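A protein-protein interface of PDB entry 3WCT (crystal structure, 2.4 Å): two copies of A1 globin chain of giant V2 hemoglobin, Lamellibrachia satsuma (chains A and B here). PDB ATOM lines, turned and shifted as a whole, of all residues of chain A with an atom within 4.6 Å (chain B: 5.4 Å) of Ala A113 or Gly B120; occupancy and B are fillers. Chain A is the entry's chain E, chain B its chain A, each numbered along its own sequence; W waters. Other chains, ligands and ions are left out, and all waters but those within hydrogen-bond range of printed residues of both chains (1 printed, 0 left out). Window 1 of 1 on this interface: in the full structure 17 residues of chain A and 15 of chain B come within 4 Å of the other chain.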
ATOM      1  N   TYR A  38      22.161 -32.810 -13.446  1.00  0.00           N
ATOM      2  CA  TYR A  38      21.096 -33.726 -13.877  1.00  0.00           C
ATOM      3  C   TYR A  38      21.598 -35.167 -13.782  1.00  0.00           C
ATOM      4  O   TYR A  38      20.838 -36.071 -13.452  1.00  0.00           O
ATOM      5  CB  TYR A  38      20.666 -33.450 -15.332  1.00  0.00           C
ATOM      6  CG  TYR A  38      19.757 -32.250 -15.550  1.00  0.00           C
ATOM      7  CD1 TYR A  38      19.305 -31.476 -14.481  1.00  0.00           C
ATOM      8  CD2 TYR A  38      19.344 -31.894 -16.841  1.00  0.00           C
ATOM      9  CE1 TYR A  38      18.467 -30.380 -14.687  1.00  0.00           C
ATOM     10  CE2 TYR A  38      18.506 -30.802 -17.059  1.00  0.00           C
ATOM     11  CZ  TYR A  38      18.071 -30.050 -15.978  1.00  0.00           C
ATOM     12  OH  TYR A  38      17.233 -28.973 -16.187  1.00  0.00           O
ATOM     13  N   LYS A 109      17.694 -32.525 -22.111  1.00  0.00           N
ATOM     14  CA  LYS A 109      16.909 -31.900 -21.051  1.00  0.00           C
ATOM     15  C   LYS A 109      17.614 -30.619 -20.598  1.00  0.00           C
ATOM     16  O   LYS A 109      16.982 -29.586 -20.389  1.00  0.00           O
ATOM     17  CB  LYS A 109      16.757 -32.849 -19.854  1.00  0.00           C
ATOM     18  CG  LYS A 109      15.436 -33.642 -19.806  1.00  0.00           C
ATOM     19  CD  LYS A 109      15.362 -34.735 -20.863  1.00  0.00           C
ATOM     20  CE  LYS A 109      14.047 -35.536 -20.782  1.00  0.00           C
ATOM     21  NZ  LYS A 109      13.838 -36.214 -19.475  1.00  0.00           N
ATOM     22  N   ALA A 110      18.931 -30.697 -20.452  1.00  0.00           N
ATOM     23  CA  ALA A 110      19.703 -29.551 -20.008  1.00  0.00           C
ATOM     24  C   ALA A 110      19.680 -28.457 -21.065  1.00  0.00           C
ATOM     25  O   ALA A 110      19.585 -27.273 -20.740  1.00  0.00           O
ATOM     26  CB  ALA A 110      21.153 -29.969 -19.690  1.00  0.00           C
ATOM     27  N   LEU A 111      19.745 -28.866 -22.328  1.00  0.00           N
ATOM     28  CA  LEU A 111      19.724 -27.931 -23.438  1.00  0.00           C
ATOM     29  C   LEU A 111      18.435 -27.131 -23.407  1.00  0.00           C
ATOM     30  O   LEU A 111      18.455 -25.920 -23.626  1.00  0.00           O
ATOM     31  CB  LEU A 111      19.841 -28.668 -24.778  1.00  0.00           C
ATOM     32  CG  LEU A 111      19.804 -27.814 -26.062  1.00  0.00           C
ATOM     33  CD1 LEU A 111      20.997 -26.840 -26.095  1.00  0.00           C
ATOM     34  CD2 LEU A 111      19.856 -28.737 -27.286  1.00  0.00           C
ATOM     35  N   PHE A 112      17.321 -27.802 -23.125  1.00  0.00           N
ATOM     36  CA  PHE A 112      16.021 -27.138 -23.086  1.00  0.00           C
ATOM     37  C   PHE A 112      15.901 -26.129 -21.938  1.00  0.00           C
ATOM     38  O   PHE A 112      15.417 -25.005 -22.126  1.00  0.00           O
ATOM     39  CB  PHE A 112      14.891 -28.166 -22.978  1.00  0.00           C
ATOM     40  CG  PHE A 112      14.977 -29.276 -23.987  1.00  0.00           C
ATOM     41  CD1 PHE A 112      15.530 -29.056 -25.245  1.00  0.00           C
ATOM     42  CD2 PHE A 112      14.501 -30.548 -23.675  1.00  0.00           C
ATOM     43  CE1 PHE A 112      15.613 -30.091 -26.187  1.00  0.00           C
ATOM     44  CE2 PHE A 112      14.570 -31.588 -24.590  1.00  0.00           C
ATOM     45  CZ  PHE A 112      15.131 -31.362 -25.854  1.00  0.00           C
ATOM     46  N   ALA A 113      16.361 -26.533 -20.760  1.00  0.00           N
ATOM     47  CA  ALA A 113      16.304 -25.683 -19.585  1.00  0.00           C
ATOM     48  C   ALA A 113      17.164 -24.433 -19.771  1.00  0.00           C
ATOM     49  O   ALA A 113      16.778 -23.330 -19.365  1.00  0.00           O
ATOM     50  CB  ALA A 113      16.761 -26.458 -18.367  1.00  0.00           C
ATOM     51  N   THR A 114      18.328 -24.621 -20.385  1.00  0.00           N
ATOM     52  CA  THR A 114      19.236 -23.525 -20.636  1.00  0.00           C
ATOM     53  C   THR A 114      18.663 -22.576 -21.702  1.00  0.00           C
ATOM     54  O   THR A 114      18.526 -21.377 -21.452  1.00  0.00           O
ATOM     55  CB  THR A 114      20.609 -24.039 -21.101  1.00  0.00           C
ATOM     56  OG1 THR A 114      21.051 -25.073 -20.215  1.00  0.00           O
ATOM     57  CG2 THR A 114      21.629 -22.915 -21.083  1.00  0.00           C
ATOM     58  N   VAL A 115      18.318 -23.103 -22.876  1.00  0.00           N
ATOM     59  CA  VAL A 115      17.778 -22.244 -23.934  1.00  0.00           C
ATOM     60  C   VAL A 115      16.480 -21.579 -23.503  1.00  0.00           C
ATOM     61  O   VAL A 115      16.319 -20.371 -23.652  1.00  0.00           O
ATOM     62  CB  VAL A 115      17.553 -23.024 -25.262  1.00  0.00           C
ATOM     63  CG1 VAL A 115      16.910 -22.110 -26.320  1.00  0.00           C
ATOM     64  CG2 VAL A 115      18.904 -23.557 -25.781  1.00  0.00           C
ATOM     65  N   GLY A 116      15.563 -22.366 -22.952  1.00  0.00           N
ATOM     66  CA  GLY A 116      14.294 -21.821 -22.502  1.00  0.00           C
ATOM     67  C   GLY A 116      14.487 -20.823 -21.378  1.00  0.00           C
ATOM     68  O   GLY A 116      13.788 -19.805 -21.310  1.00  0.00           O
ATOM     69  N   GLY A 117      15.439 -21.118 -20.496  1.00  0.00           N
ATOM     70  CA  GLY A 117      15.718 -20.232 -19.370  1.00  0.00           C
ATOM     71  C   GLY A 117      16.252 -18.897 -19.850  1.00  0.00           C
ATOM     72  O   GLY A 117      16.013 -17.860 -19.250  1.00  0.00           O
ATOM     73  N   VAL B 115       7.251 -21.944 -16.723  1.00  0.00           N
ATOM     74  CA  VAL B 115       8.029 -21.904 -15.495  1.00  0.00           C
ATOM     75  C   VAL B 115       9.508 -21.739 -15.834  1.00  0.00           C
ATOM     76  O   VAL B 115      10.207 -20.940 -15.217  1.00  0.00           O
ATOM     77  CB  VAL B 115       7.836 -23.202 -14.642  1.00  0.00           C
ATOM     78  CG1 VAL B 115       8.796 -23.213 -13.457  1.00  0.00           C
ATOM     79  CG2 VAL B 115       6.396 -23.290 -14.141  1.00  0.00           C
ATOM     80  N   GLY B 116       9.978 -22.492 -16.820  1.00  0.00           N
ATOM     81  CA  GLY B 116      11.377 -22.405 -17.200  1.00  0.00           C
ATOM     82  C   GLY B 116      11.779 -21.023 -17.700  1.00  0.00           C
ATOM     83  O   GLY B 116      12.843 -20.511 -17.362  1.00  0.00           O
ATOM     84  N   GLY B 117      10.924 -20.419 -18.514  1.00  0.00           N
ATOM     85  CA  GLY B 117      11.211 -19.104 -19.053  1.00  0.00           C
ATOM     86  C   GLY B 117      11.244 -18.034 -17.983  1.00  0.00           C
ATOM     87  O   GLY B 117      12.062 -17.124 -18.034  1.00  0.00           O
ATOM     88  N   GLN B 118      10.364 -18.155 -17.000  1.00  0.00           N
ATOM     89  CA  GLN B 118      10.286 -17.190 -15.917  1.00  0.00           C
ATOM     90  C   GLN B 118      11.312 -17.419 -14.794  1.00  0.00           C
ATOM     91  O   GLN B 118      11.721 -16.473 -14.125  1.00  0.00           O
ATOM     92  CB  GLN B 118       8.872 -17.206 -15.341  1.00  0.00           C
ATOM     93  CG  GLN B 118       8.591 -16.127 -14.338  1.00  0.00           C
ATOM     94  CD  GLN B 118       8.564 -14.748 -14.965  1.00  0.00           C
ATOM     95  OE1 GLN B 118       7.760 -14.475 -15.848  1.00  0.00           O
ATOM     96  NE2 GLN B 118       9.447 -13.868 -14.502  1.00  0.00           N
ATOM     97  N   PHE B 119      11.727 -18.667 -14.591  1.00  0.00           N
ATOM     98  CA  PHE B 119      12.677 -18.984 -13.527  1.00  0.00           C
ATOM     99  C   PHE B 119      14.101 -18.865 -13.997  1.00  0.00           C
ATOM    100  O   PHE B 119      14.986 -18.519 -13.227  1.00  0.00           O
ATOM    101  CB  PHE B 119      12.465 -20.405 -12.981  1.00  0.00           C
ATOM    102  CG  PHE B 119      13.346 -20.737 -11.796  1.00  0.00           C
ATOM    103  CD1 PHE B 119      13.049 -20.246 -10.530  1.00  0.00           C
ATOM    104  CD2 PHE B 119      14.499 -21.507 -11.957  1.00  0.00           C
ATOM    105  CE1 PHE B 119      13.890 -20.514  -9.439  1.00  0.00           C
ATOM    106  CE2 PHE B 119      15.342 -21.778 -10.879  1.00  0.00           C
ATOM    107  CZ  PHE B 119      15.044 -21.285  -9.622  1.00  0.00           C
ATOM    108  N   GLY B 120      14.335 -19.170 -15.260  1.00  0.00           N
ATOM    109  CA  GLY B 120      15.683 -19.076 -15.760  1.00  0.00           C
ATOM    110  C   GLY B 120      16.318 -20.417 -16.061  1.00  0.00           C
ATOM    111  O   GLY B 120      15.670 -21.474 -16.059  1.00  0.00           O
ATOM    112  N   VAL B 121      17.619 -20.336 -16.294  1.00  0.00           N
ATOM    113  CA  VAL B 121      18.481 -21.439 -16.660  1.00  0.00           C
ATOM    114  C   VAL B 121      18.660 -22.577 -15.655  1.00  0.00           C
ATOM    115  O   VAL B 121      19.095 -23.660 -16.031  1.00  0.00           O
ATOM    116  CB  VAL B 121      19.863 -20.861 -17.042  1.00  0.00           C
ATOM    117  CG1 VAL B 121      20.833 -21.961 -17.395  1.00  0.00           C
ATOM    118  CG2 VAL B 121      19.698 -19.921 -18.211  1.00  0.00           C
ATOM    119  N   CYS B 122      18.351 -22.349 -14.383  1.00  0.00           N
ATOM    120  CA  CYS B 122      18.517 -23.414 -13.397  1.00  0.00           C
ATOM    121  C   CYS B 122      17.233 -24.228 -13.249  1.00  0.00           C
ATOM    122  O   CYS B 122      17.104 -25.053 -12.349  1.00  0.00           O
ATOM    123  CB  CYS B 122      18.945 -22.833 -12.049  1.00  0.00           C
ATOM    124  SG  CYS B 122      20.383 -21.721 -12.180  1.00  0.00           S
ATOM    125  N   PHE B 123      16.284 -23.977 -14.146  1.00  0.00           N
ATOM    126  CA  PHE B 123      15.014 -24.696 -14.168  1.00  0.00           C
ATOM    127  C   PHE B 123      15.381 -26.182 -14.184  1.00  0.00           C
ATOM    128  O   PHE B 123      16.276 -26.588 -14.916  1.00  0.00           O
ATOM    129  CB  PHE B 123      14.263 -24.319 -15.437  1.00  0.00           C
ATOM    130  CG  PHE B 123      13.033 -25.130 -15.689  1.00  0.00           C
ATOM    131  CD1 PHE B 123      11.939 -25.033 -14.842  1.00  0.00           C
ATOM    132  CD2 PHE B 123      12.938 -25.935 -16.829  1.00  0.00           C
ATOM    133  CE1 PHE B 123      10.766 -25.707 -15.121  1.00  0.00           C
ATOM    134  CE2 PHE B 123      11.773 -26.613 -17.120  1.00  0.00           C
ATOM    135  CZ  PHE B 123      10.676 -26.503 -16.268  1.00  0.00           C
ATOM    136  N   LEU B 125      14.214 -29.308 -15.421  1.00  0.00           N
ATOM    137  CA  LEU B 125      13.234 -29.961 -16.280  1.00  0.00           C
ATOM    138  C   LEU B 125      12.918 -31.430 -15.901  1.00  0.00           C
ATOM    139  O   LEU B 125      11.746 -31.803 -15.840  1.00  0.00           O
ATOM    140  CB  LEU B 125      13.660 -29.865 -17.757  1.00  0.00           C
ATOM    141  CG  LEU B 125      12.768 -30.549 -18.809  1.00  0.00           C
ATOM    142  CD1 LEU B 125      11.356 -29.988 -18.740  1.00  0.00           C
ATOM    143  CD2 LEU B 125      13.339 -30.328 -20.194  1.00  0.00           C
HETATM  144  O   HOH W   1      19.066 -26.884 -14.241  1.00  0.00           O
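O of Phe B123 is in hydrogen-bond range of OH of Tyr A38 (2.9 Å). The side-chain hydroxyl of Tyr A38 sits at hydrogen-bond distance from the backbone NH of Leu B125, at 3.1 Å.
The side-chain hydroxyl (OG1) of Thr A114 lies within hydrogen-bond range of the backbone carbonyl oxygen (O) of Ala A110, 2.7 Å away.
O of Lys A109 touches CD2 of Leu B125, at 3.7 Å. Leu B125 touches Phe A112 (CD2 to CD2, 3.7 Å). Gly B120 touches Ala A113. Ala A113 touches Val B121. O of Phe B123 touches CB of Ala A113, at 3.5 Å. O of Thr A114 touches CG2 of Val B121, 3.7 Å away. CA of Gly B117 touches O of Gly A116, at 3.5 Å. CA of Gly A117 touches O of Gly B116, at 3.5 Å. Gly A117 touches Gly B120. Gly A117 touches Val B121 (CA to N, 3.6 Å).
Of chain B, only Gly B120 (3.9 Å), Val B121 (3.7 Å) and Phe B123 (3.5 Å) come within 4 Å of Ala A113. Of chain A, only Ala A113 and Gly A117 come within 4 Å of Gly B120. Of the printed residues of chain B, Phe A112 touches Leu B125. Printed residues of chain B within 4 Å of Thr A114: Val B121. Of the printed residues of chain B, Tyr A38 touches Phe B123 (2.9 Å) and Leu B125 (3.1 Å). Of the printed residues of chain B, Gly A117 touches Gly B116, Gly B120 and Val B121. The nearest printed residue of chain A that does not touch Gly B120 is Gly A116 (5.5 Å).
Printed residues of chain A that touch a printed residue of chain B: Tyr A38, Lys A109, Phe A112, Ala A113, Thr A114, Gly A116 and Gly A117. Printed residues of chain B that touch a printed residue of chain A: Gly B116, Gly B117, Gly B120, Val B121, Phe B123 and Leu B125. Hydrophobic or aromatic side chains of chain B within 4 Å of the printed part of chain A: Val B121 and Leu B125. Among the printed residues, 12 pairs touch across the chains. Among the printed residues, no Asp or Glu carboxylate lies within 4 Å of a Lys or Arg side-chain nitrogen of the other chain.
Gly A116 touches Gly B117, and with the chains exchanged Gly A117 touches Gly B116. Positions printed for both chains: 115, 116 and 117.
Water W1 lies within hydrogen-bond range of the backbone carbonyl oxygen of Phe B123 (2.9 Å), the backbone carbonyl oxygen of Cys B122 (3.3 Å) and the side-chain hydroxyl of Tyr A38 (3.4 Å).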
